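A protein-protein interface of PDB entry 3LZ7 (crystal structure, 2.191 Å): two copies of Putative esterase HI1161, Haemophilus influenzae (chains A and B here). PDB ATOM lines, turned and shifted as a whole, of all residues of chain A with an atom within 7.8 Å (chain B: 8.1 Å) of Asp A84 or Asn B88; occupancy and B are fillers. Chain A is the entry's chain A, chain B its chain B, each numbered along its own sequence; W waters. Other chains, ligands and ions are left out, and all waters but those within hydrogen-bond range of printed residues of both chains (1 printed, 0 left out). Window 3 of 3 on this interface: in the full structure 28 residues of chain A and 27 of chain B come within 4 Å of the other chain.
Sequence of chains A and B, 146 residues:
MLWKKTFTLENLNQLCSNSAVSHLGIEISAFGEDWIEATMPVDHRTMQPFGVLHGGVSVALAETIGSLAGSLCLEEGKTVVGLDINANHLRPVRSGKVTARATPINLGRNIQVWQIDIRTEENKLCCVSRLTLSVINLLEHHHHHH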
ATOM      1  N   GLU A  63     -33.859  29.147   4.074  1.00  0.00           N
ATOM      2  CA  GLU A  63     -33.752  28.512   5.371  1.00  0.00           C
ATOM      3  C   GLU A  63     -35.145  28.219   5.909  1.00  0.00           C
ATOM      4  O   GLU A  63     -35.362  27.183   6.535  1.00  0.00           O
ATOM      5  CB  GLU A  63     -32.940  29.356   6.362  1.00  0.00           C
ATOM      6  CG  GLU A  63     -32.948  28.751   7.752  1.00  0.00           C
ATOM      7  CD  GLU A  63     -31.607  28.876   8.463  1.00  0.00           C
ATOM      8  OE1 GLU A  63     -30.643  29.380   7.836  1.00  0.00           O
ATOM      9  OE2 GLU A  63     -31.527  28.468   9.646  1.00  0.00           O
ATOM     10  N   VAL A  81     -33.186  21.828  13.779  1.00  0.00           N
ATOM     11  CA  VAL A  81     -32.550  23.085  14.131  1.00  0.00           C
ATOM     12  C   VAL A  81     -31.526  23.385  13.036  1.00  0.00           C
ATOM     13  O   VAL A  81     -30.731  22.521  12.683  1.00  0.00           O
ATOM     14  CB  VAL A  81     -31.819  22.960  15.484  1.00  0.00           C
ATOM     15  CG1 VAL A  81     -30.909  24.142  15.717  1.00  0.00           C
ATOM     16  CG2 VAL A  81     -32.820  22.828  16.611  1.00  0.00           C
ATOM     17  N   GLY A  82     -31.546  24.588  12.480  1.00  0.00           N
ATOM     18  CA  GLY A  82     -30.606  24.936  11.411  1.00  0.00           C
ATOM     19  C   GLY A  82     -29.167  25.007  11.887  1.00  0.00           C
ATOM     20  O   GLY A  82     -28.884  25.656  12.890  1.00  0.00           O
ATOM     21  N   LEU A  83     -28.259  24.322  11.198  1.00  0.00           N
ATOM     22  CA  LEU A  83     -26.854  24.317  11.594  1.00  0.00           C
ATOM     23  C   LEU A  83     -26.098  25.262  10.714  1.00  0.00           C
ATOM     24  O   LEU A  83     -25.309  26.092  11.187  1.00  0.00           O
ATOM     25  CB  LEU A  83     -26.212  22.924  11.461  1.00  0.00           C
ATOM     26  CG  LEU A  83     -26.604  21.831  12.455  1.00  0.00           C
ATOM     27  CD1 LEU A  83     -25.712  20.624  12.245  1.00  0.00           C
ATOM     28  CD2 LEU A  83     -26.548  22.314  13.937  1.00  0.00           C
ATOM     29  N   ASP A  84     -26.329  25.129   9.418  1.00  0.00           N
ATOM     30  CA  ASP A  84     -25.624  25.974   8.471  1.00  0.00           C
ATOM     31  C   ASP A  84     -26.297  26.060   7.132  1.00  0.00           C
ATOM     32  O   ASP A  84     -27.119  25.224   6.763  1.00  0.00           O
ATOM     33  CB  ASP A  84     -24.143  25.572   8.324  1.00  0.00           C
ATOM     34  CG  ASP A  84     -23.946  24.239   7.666  1.00  0.00           C
ATOM     35  OD1 ASP A  84     -24.438  24.039   6.536  1.00  0.00           O
ATOM     36  OD2 ASP A  84     -23.236  23.392   8.268  1.00  0.00           O
ATOM     37  N   ILE A  85     -25.945  27.085   6.384  1.00  0.00           N
ATOM     38  CA  ILE A  85     -26.574  27.247   5.092  1.00  0.00           C
ATOM     39  C   ILE A  85     -25.565  27.897   4.188  1.00  0.00           C
ATOM     40  O   ILE A  85     -24.706  28.658   4.644  1.00  0.00           O
ATOM     41  CB  ILE A  85     -27.877  28.098   5.201  1.00  0.00           C
ATOM     42  CG1 ILE A  85     -28.610  28.149   3.854  1.00  0.00           C
ATOM     43  CG2 ILE A  85     -27.551  29.489   5.697  1.00  0.00           C
ATOM     44  CD1 ILE A  85     -30.103  28.460   3.958  1.00  0.00           C
ATOM     45  N   ASN A  86     -25.635  27.581   2.903  1.00  0.00           N
ATOM     46  CA  ASN A  86     -24.824  28.314   1.940  1.00  0.00           C
ATOM     47  C   ASN A  86     -25.658  28.560   0.694  1.00  0.00           C
ATOM     48  O   ASN A  86     -26.649  27.882   0.485  1.00  0.00           O
ATOM     49  CB  ASN A  86     -23.533  27.567   1.644  1.00  0.00           C
ATOM     50  CG  ASN A  86     -23.776  26.204   1.032  1.00  0.00           C
ATOM     51  OD1 ASN A  86     -24.466  26.078   0.015  1.00  0.00           O
ATOM     52  ND2 ASN A  86     -23.195  25.177   1.637  1.00  0.00           N
ATOM     53  N   GLN A 112     -29.877  16.177   8.655  1.00  0.00           N
ATOM     54  CA  GLN A 112     -30.513  16.235   7.336  1.00  0.00           C
ATOM     55  C   GLN A 112     -29.819  17.270   6.446  1.00  0.00           C
ATOM     56  O   GLN A 112     -29.352  18.298   6.935  1.00  0.00           O
ATOM     57  CB  GLN A 112     -31.996  16.594   7.449  1.00  0.00           C
ATOM     58  CG  GLN A 112     -32.843  15.646   8.289  1.00  0.00           C
ATOM     59  CD  GLN A 112     -34.301  16.111   8.358  1.00  0.00           C
ATOM     60  OE1 GLN A 112     -35.175  15.436   8.920  1.00  0.00           O
ATOM     61  NE2 GLN A 112     -34.562  17.264   7.780  1.00  0.00           N
ATOM     62  N   VAL A 113     -29.750  16.996   5.143  1.00  0.00           N
ATOM     63  CA  VAL A 113     -29.226  17.966   4.184  1.00  0.00           C
ATOM     64  C   VAL A 113     -30.288  18.240   3.118  1.00  0.00           C
ATOM     65  O   VAL A 113     -30.808  17.310   2.501  1.00  0.00           O
ATOM     66  CB  VAL A 113     -27.935  17.457   3.513  1.00  0.00           C
ATOM     67  CG1 VAL A 113     -27.319  18.552   2.646  1.00  0.00           C
ATOM     68  CG2 VAL A 113     -26.929  16.955   4.561  1.00  0.00           C
ATOM     69  N   TRP A 114     -30.621  19.512   2.913  1.00  0.00           N
ATOM     70  CA  TRP A 114     -31.689  19.886   1.985  1.00  0.00           C
ATOM     71  C   TRP A 114     -31.161  20.778   0.884  1.00  0.00           C
ATOM     72  O   TRP A 114     -30.269  21.598   1.111  1.00  0.00           O
ATOM     73  CB  TRP A 114     -32.825  20.628   2.720  1.00  0.00           C
ATOM     74  CG  TRP A 114     -33.679  19.726   3.522  1.00  0.00           C
ATOM     75  CD1 TRP A 114     -33.436  19.274   4.796  1.00  0.00           C
ATOM     76  CD2 TRP A 114     -34.917  19.128   3.112  1.00  0.00           C
ATOM     77  NE1 TRP A 114     -34.450  18.436   5.197  1.00  0.00           N
ATOM     78  CE2 TRP A 114     -35.373  18.332   4.187  1.00  0.00           C
ATOM     79  CE3 TRP A 114     -35.686  19.194   1.946  1.00  0.00           C
ATOM     80  CZ2 TRP A 114     -36.559  17.598   4.125  1.00  0.00           C
ATOM     81  CZ3 TRP A 114     -36.863  18.471   1.890  1.00  0.00           C
ATOM     82  CH2 TRP A 114     -37.288  17.677   2.973  1.00  0.00           C
ATOM     83  N   SER A 129     -29.173  26.973  -2.939  1.00  0.00           N
ATOM     84  CA  SER A 129     -28.790  26.942  -1.547  1.00  0.00           C
ATOM     85  C   SER A 129     -28.760  25.500  -1.094  1.00  0.00           C
ATOM     86  O   SER A 129     -29.485  24.658  -1.635  1.00  0.00           O
ATOM     87  CB  SER A 129     -29.836  27.723  -0.736  1.00  0.00           C
ATOM     88  OG  SER A 129     -29.658  27.560   0.647  1.00  0.00           O
ATOM     89  N   ARG A 130     -27.927  25.218  -0.097  1.00  0.00           N
ATOM     90  CA  ARG A 130     -27.951  23.926   0.570  1.00  0.00           C
ATOM     91  C   ARG A 130     -27.974  24.160   2.071  1.00  0.00           C
ATOM     92  O   ARG A 130     -27.208  24.983   2.606  1.00  0.00           O
ATOM     93  CB  ARG A 130     -26.739  23.080   0.173  1.00  0.00           C
ATOM     94  CG  ARG A 130     -26.957  21.586   0.333  1.00  0.00           C
ATOM     95  CD  ARG A 130     -25.828  20.783  -0.335  1.00  0.00           C
ATOM     96  NE  ARG A 130     -24.555  21.038   0.325  1.00  0.00           N
ATOM     97  CZ  ARG A 130     -23.565  21.763  -0.192  1.00  0.00           C
ATOM     98  NH1 ARG A 130     -23.669  22.281  -1.402  1.00  0.00           N
ATOM     99  NH2 ARG A 130     -22.456  21.953   0.504  1.00  0.00           N
ATOM    100  N   LEU A 131     -28.844  23.433   2.755  1.00  0.00           N
ATOM    101  CA  LEU A 131     -29.062  23.664   4.172  1.00  0.00           C
ATOM    102  C   LEU A 131     -28.754  22.399   4.976  1.00  0.00           C
ATOM    103  O   LEU A 131     -29.162  21.302   4.588  1.00  0.00           O
ATOM    104  CB  LEU A 131     -30.524  24.059   4.383  1.00  0.00           C
ATOM    105  CG  LEU A 131     -31.053  24.094   5.816  1.00  0.00           C
ATOM    106  CD1 LEU A 131     -30.376  25.205   6.629  1.00  0.00           C
ATOM    107  CD2 LEU A 131     -32.555  24.312   5.758  1.00  0.00           C
ATOM    108  N   THR A 132     -28.045  22.547   6.096  1.00  0.00           N
ATOM    109  CA  THR A 132     -27.735  21.405   6.954  1.00  0.00           C
ATOM    110  C   THR A 132     -28.506  21.541   8.266  1.00  0.00           C
ATOM    111  O   THR A 132     -28.422  22.569   8.940  1.00  0.00           O
ATOM    112  CB  THR A 132     -26.218  21.295   7.249  1.00  0.00           C
ATOM    113  OG1 THR A 132     -25.485  21.336   6.024  1.00  0.00           O
ATOM    114  CG2 THR A 132     -25.887  19.984   7.988  1.00  0.00           C
ATOM    115  N   LEU A 133     -29.288  20.525   8.603  1.00  0.00           N
ATOM    116  CA  LEU A 133     -30.103  20.560   9.815  1.00  0.00           C
ATOM    117  C   LEU A 133     -29.711  19.464  10.795  1.00  0.00           C
ATOM    118  O   LEU A 133     -29.290  18.380  10.398  1.00  0.00           O
ATOM    119  CB  LEU A 133     -31.579  20.370   9.475  1.00  0.00           C
ATOM    120  CG  LEU A 133     -32.246  21.302   8.471  1.00  0.00           C
ATOM    121  CD1 LEU A 133     -33.650  20.795   8.172  1.00  0.00           C
ATOM    122  CD2 LEU A 133     -32.283  22.682   9.068  1.00  0.00           C
ATOM    123  N   SER A 134     -29.910  19.755  12.075  1.00  0.00           N
ATOM    124  CA  SER A 134     -29.767  18.779  13.150  1.00  0.00           C
ATOM    125  C   SER A 134     -31.149  18.270  13.563  1.00  0.00           C
ATOM    126  O   SER A 134     -32.064  19.064  13.714  1.00  0.00           O
ATOM    127  CB  SER A 134     -29.152  19.484  14.354  1.00  0.00           C
ATOM    128  OG  SER A 134     -28.674  18.548  15.282  1.00  0.00           O
ATOM    129  N   GLY B  55     -32.502  32.111  11.818  1.00  0.00           N
ATOM    130  CA  GLY B  55     -31.143  32.026  11.315  1.00  0.00           C
ATOM    131  C   GLY B  55     -31.036  32.544   9.900  1.00  0.00           C
ATOM    132  O   GLY B  55     -29.994  33.046   9.483  1.00  0.00           O
ATOM    133  N   SER B  58     -30.551  36.336  10.259  1.00  0.00           N
ATOM    134  CA  SER B  58     -29.139  36.618  10.590  1.00  0.00           C
ATOM    135  C   SER B  58     -28.303  36.676   9.324  1.00  0.00           C
ATOM    136  O   SER B  58     -27.429  37.528   9.186  1.00  0.00           O
ATOM    137  CB  SER B  58     -28.538  35.527  11.486  1.00  0.00           C
ATOM    138  OG  SER B  58     -29.349  35.300  12.598  1.00  0.00           O
ATOM    139  N   VAL B  59     -28.569  35.760   8.390  1.00  0.00           N
ATOM    140  CA  VAL B  59     -27.875  35.818   7.107  1.00  0.00           C
ATOM    141  C   VAL B  59     -28.219  37.093   6.332  1.00  0.00           C
ATOM    142  O   VAL B  59     -27.353  37.691   5.682  1.00  0.00           O
ATOM    143  CB  VAL B  59     -28.159  34.565   6.245  1.00  0.00           C
ATOM    144  CG1 VAL B  59     -27.408  34.650   4.926  1.00  0.00           C
ATOM    145  CG2 VAL B  59     -27.762  33.326   7.016  1.00  0.00           C
ATOM    146  N   ASN B  86     -22.221  31.951   2.970  1.00  0.00           N
ATOM    147  CA  ASN B  86     -22.455  30.796   3.819  1.00  0.00           C
ATOM    148  C   ASN B  86     -22.397  31.241   5.277  1.00  0.00           C
ATOM    149  O   ASN B  86     -21.802  32.276   5.589  1.00  0.00           O
ATOM    150  CB  ASN B  86     -21.427  29.704   3.541  1.00  0.00           C
ATOM    151  CG  ASN B  86     -20.031  30.154   3.826  1.00  0.00           C
ATOM    152  OD1 ASN B  86     -19.711  30.546   4.953  1.00  0.00           O
ATOM    153  ND2 ASN B  86     -19.173  30.108   2.804  1.00  0.00           N
ATOM    154  N   ALA B  87     -23.013  30.463   6.158  1.00  0.00           N
ATOM    155  CA  ALA B  87     -23.075  30.813   7.571  1.00  0.00           C
ATOM    156  C   ALA B  87     -23.263  29.570   8.409  1.00  0.00           C
ATOM    157  O   ALA B  87     -23.861  28.585   7.952  1.00  0.00           O
ATOM    158  CB  ALA B  87     -24.225  31.811   7.835  1.00  0.00           C
ATOM    159  N   ASN B  88     -22.725  29.613   9.626  1.00  0.00           N
ATOM    160  CA  ASN B  88     -23.039  28.630  10.653  1.00  0.00           C
ATOM    161  C   ASN B  88     -23.785  29.352  11.764  1.00  0.00           C
ATOM    162  O   ASN B  88     -23.380  30.457  12.173  1.00  0.00           O
ATOM    163  CB  ASN B  88     -21.769  27.985  11.225  1.00  0.00           C
ATOM    164  CG  ASN B  88     -21.253  26.838  10.359  1.00  0.00           C
ATOM    165  OD1 ASN B  88     -20.608  27.060   9.341  1.00  0.00           O
ATOM    166  ND2 ASN B  88     -21.559  25.612  10.755  1.00  0.00           N
ATOM    167  N   HIS B  89     -24.876  28.748  12.231  1.00  0.00           N
ATOM    168  CA  HIS B  89     -25.596  29.267  13.384  1.00  0.00           C
ATOM    169  C   HIS B  89     -25.088  28.544  14.631  1.00  0.00           C
ATOM    170  O   HIS B  89     -25.134  27.322  14.706  1.00  0.00           O
ATOM    171  CB  HIS B  89     -27.109  29.117  13.171  1.00  0.00           C
ATOM    172  CG  HIS B  89     -27.569  29.713  11.877  1.00  0.00           C
ATOM    173  ND1 HIS B  89     -28.049  28.952  10.830  1.00  0.00           N
ATOM    174  CD2 HIS B  89     -27.542  30.988  11.430  1.00  0.00           C
ATOM    175  CE1 HIS B  89     -28.321  29.734   9.805  1.00  0.00           C
ATOM    176  NE2 HIS B  89     -28.022  30.976  10.142  1.00  0.00           N
ATOM    177  N   LEU B  90     -24.562  29.304  15.587  1.00  0.00           N
ATOM    178  CA  LEU B  90     -23.774  28.716  16.670  1.00  0.00           C
ATOM    179  C   LEU B  90     -24.601  28.578  17.925  1.00  0.00           C
ATOM    180  O   LEU B  90     -24.425  27.637  18.690  1.00  0.00           O
ATOM    181  CB  LEU B  90     -22.521  29.559  16.941  1.00  0.00           C
ATOM    182  CG  LEU B  90     -21.706  29.746  15.656  1.00  0.00           C
ATOM    183  CD1 LEU B  90     -20.648  30.792  15.852  1.00  0.00           C
ATOM    184  CD2 LEU B  90     -21.083  28.413  15.202  1.00  0.00           C
ATOM    185  N   ARG B  91     -25.517  29.513  18.136  1.00  0.00           N
ATOM    186  CA  ARG B  91     -26.381  29.426  19.303  1.00  0.00           C
ATOM    187  C   ARG B  91     -27.678  30.193  19.099  1.00  0.00           C
ATOM    188  O   ARG B  91     -27.714  31.164  18.348  1.00  0.00           O
ATOM    189  CB  ARG B  91     -25.649  29.954  20.538  1.00  0.00           C
ATOM    190  CG  ARG B  91     -25.603  31.454  20.636  1.00  0.00           C
ATOM    191  CD  ARG B  91     -24.720  31.860  21.800  1.00  0.00           C
ATOM    192  NE  ARG B  91     -23.382  31.296  21.644  1.00  0.00           N
ATOM    193  CZ  ARG B  91     -22.675  30.764  22.636  1.00  0.00           C
ATOM    194  NH1 ARG B  91     -23.182  30.717  23.863  1.00  0.00           N
ATOM    195  NH2 ARG B  91     -21.461  30.278  22.399  1.00  0.00           N
ATOM    196  N   ILE B 116     -18.203  38.045   8.366  1.00  0.00           N
ATOM    197  CA  ILE B 116     -19.174  38.669   9.249  1.00  0.00           C
ATOM    198  C   ILE B 116     -19.325  37.844  10.527  1.00  0.00           C
ATOM    199  O   ILE B 116     -19.571  36.635  10.475  1.00  0.00           O
ATOM    200  CB  ILE B 116     -20.546  38.867   8.584  1.00  0.00           C
ATOM    201  CG1 ILE B 116     -20.444  39.819   7.383  1.00  0.00           C
ATOM    202  CG2 ILE B 116     -21.569  39.396   9.602  1.00  0.00           C
ATOM    203  CD1 ILE B 116     -20.220  39.093   6.030  1.00  0.00           C
ATOM    204  N   ILE B 118     -21.527  37.751  14.046  1.00  0.00           N
ATOM    205  CA  ILE B 118     -22.705  38.313  14.694  1.00  0.00           C
ATOM    206  C   ILE B 118     -22.683  37.899  16.159  1.00  0.00           C
ATOM    207  O   ILE B 118     -22.513  36.719  16.468  1.00  0.00           O
ATOM    208  CB  ILE B 118     -24.000  37.839  14.023  1.00  0.00           C
ATOM    209  CG1 ILE B 118     -23.929  38.084  12.509  1.00  0.00           C
ATOM    210  CG2 ILE B 118     -25.232  38.537  14.650  1.00  0.00           C
ATOM    211  CD1 ILE B 118     -25.209  37.751  11.757  1.00  0.00           C
ATOM    212  N   LEU B 125     -20.726  35.075  20.469  1.00  0.00           N
ATOM    213  CA  LEU B 125     -20.832  34.803  19.051  1.00  0.00           C
ATOM    214  C   LEU B 125     -22.033  33.894  18.794  1.00  0.00           C
ATOM    215  O   LEU B 125     -22.130  32.802  19.359  1.00  0.00           O
ATOM    216  CB  LEU B 125     -19.536  34.155  18.585  1.00  0.00           C
ATOM    217  CG  LEU B 125     -19.108  34.272  17.131  1.00  0.00           C
ATOM    218  CD1 LEU B 125     -19.102  35.730  16.673  1.00  0.00           C
ATOM    219  CD2 LEU B 125     -17.719  33.637  16.975  1.00  0.00           C
ATOM    220  N   CYS B 126     -22.969  34.348  17.965  1.00  0.00           N
ATOM    221  CA  CYS B 126     -24.136  33.517  17.665  1.00  0.00           C
ATOM    222  C   CYS B 126     -24.210  33.045  16.214  1.00  0.00           C
ATOM    223  O   CYS B 126     -24.953  32.110  15.905  1.00  0.00           O
ATOM    224  CB  CYS B 126     -25.439  34.204  18.061  1.00  0.00           C
ATOM    225  SG  CYS B 126     -25.819  35.671  17.103  1.00  0.00           S
ATOM    226  N   CYS B 127     -23.442  33.672  15.332  1.00  0.00           N
ATOM    227  CA  CYS B 127     -23.486  33.296  13.914  1.00  0.00           C
ATOM    228  C   CYS B 127     -22.217  33.779  13.259  1.00  0.00           C
ATOM    229  O   CYS B 127     -21.754  34.881  13.556  1.00  0.00           O
ATOM    230  CB  CYS B 127     -24.712  33.932  13.222  1.00  0.00           C
ATOM    231  SG  CYS B 127     -24.848  33.577  11.434  1.00  0.00           S
ATOM    232  N   VAL B 128     -21.610  32.939  12.425  1.00  0.00           N
ATOM    233  CA  VAL B 128     -20.470  33.369  11.606  1.00  0.00           C
ATOM    234  C   VAL B 128     -20.779  33.130  10.138  1.00  0.00           C
ATOM    235  O   VAL B 128     -21.443  32.155   9.792  1.00  0.00           O
ATOM    236  CB  VAL B 128     -19.157  32.647  11.962  1.00  0.00           C
ATOM    237  CG1 VAL B 128     -18.667  33.110  13.320  1.00  0.00           C
ATOM    238  CG2 VAL B 128     -19.353  31.117  11.932  1.00  0.00           C
ATOM    239  N   SER B 129     -20.265  34.011   9.283  1.00  0.00           N
ATOM    240  CA  SER B 129     -20.648  34.053   7.878  1.00  0.00           C
ATOM    241  C   SER B 129     -19.486  34.547   7.042  1.00  0.00           C
ATOM    242  O   SER B 129     -18.720  35.428   7.452  1.00  0.00           O
ATOM    243  CB  SER B 129     -21.849  35.002   7.687  1.00  0.00           C
ATOM    244  OG  SER B 129     -22.166  35.192   6.317  1.00  0.00           O
ATOM    245  N   ARG B 130     -19.340  33.975   5.863  1.00  0.00           N
ATOM    246  CA  ARG B 130     -18.391  34.517   4.916  1.00  0.00           C
ATOM    247  C   ARG B 130     -19.157  34.894   3.664  1.00  0.00           C
ATOM    248  O   ARG B 130     -20.067  34.167   3.220  1.00  0.00           O
ATOM    249  CB  ARG B 130     -17.270  33.522   4.618  1.00  0.00           C
ATOM    250  CG  ARG B 130     -16.051  34.135   3.933  1.00  0.00           C
ATOM    251  CD  ARG B 130     -14.840  33.192   4.050  1.00  0.00           C
ATOM    252  NE  ARG B 130     -15.078  31.982   3.279  1.00  0.00           N
ATOM    253  CZ  ARG B 130     -15.316  30.779   3.783  1.00  0.00           C
ATOM    254  NH1 ARG B 130     -15.299  30.571   5.092  1.00  0.00           N
ATOM    255  NH2 ARG B 130     -15.536  29.771   2.957  1.00  0.00           N
HETATM  256  O   HOH W   1     -23.213  25.303  13.007  1.00  0.00           O
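N of His B89 sits at hydrogen-bond distance from O of Leu A83 (2.9 Å).
O of Ile A85 sits at hydrogen-bond distance from N of Ala B87, 2.9 Å away.
The side-chain hydroxyl (OG) of Ser B129 lies within hydrogen-bond range of the backbone carbonyl oxygen (O) of Asn B86 (3.0 Å).
The backbone NH (N) of Leu A83 is in hydrogen-bond range of the backbone carbonyl oxygen (O) of Thr A132, at 2.9 Å.
O of Asn B86 lies within hydrogen-bond range of N of Arg B130 (3.0 Å).
O of Asn B88 sits close to SG of Cys B127 (3.5 Å).
O of Asp A84 lies within hydrogen-bond range of N of Thr A132.
The side-chain hydroxyl of Ser A129 lies within hydrogen-bond range of the backbone carbonyl oxygen of Asn A86 (3.0 Å).
Among the printed residues, pairs that only touch across the chains: Glu A63 with Gly B55 (3.8 Å), Glu A63 with His B89 (3.1 Å), Gly A82 with His B89 (3.9 Å), Leu A83 with Asn B88 (3.4 Å), Asp A84 with Ala B87 (3.0 Å), Asp A84 with Asn B88 (3.5 Å), Ile A85 with Asn B86 (3.2 Å) and Asn A86 with Asn B86 (3.5 Å).
Asp A84 touches just these residues of chain B: Ala B87 and Asn B88.
Asn B88 touches two residues of chain A.
Of chain A, only Asp A84 and Ile A85 come within 4 Å of Ala B87.
Of the printed residues of chain B, Ile A85 touches Asn B86 (3.2 Å) and Ala B87 (2.9 Å).
Of the printed residues of chain B, Glu A63 touches Gly B55 and His B89.
Of the printed residues of chain A, His B89 touches Glu A63, Gly A82 and Leu A83.
Ile B116 touches none of the printed residues of chain A.
Ser A134 touches none of the printed residues of chain B.
The nearest residue of chain B that does not touch Asp A84 is His B89 (4.4 Å).
Hydrophobic or aromatic side chains of chain B that line the printed part of chain A: His B89.
Among the printed residues, 10 pairs touch across the chains.
Among the printed residues, no Asp or Glu carboxylate lies within 4 Å of a Lys or Arg side-chain nitrogen of the other chain.
Asn B86 touches its own counterpart, Asn A86.
Of the 10 pairs that touch across the chains among the printed residues, 1 has its exchanged pair printed and touching as well.
Water W1 lies within hydrogen-bond range of ND2 of Asn B88 (2.8 Å), O of Leu A83 (2.9 Å) and O of His B89 (3.3 Å).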
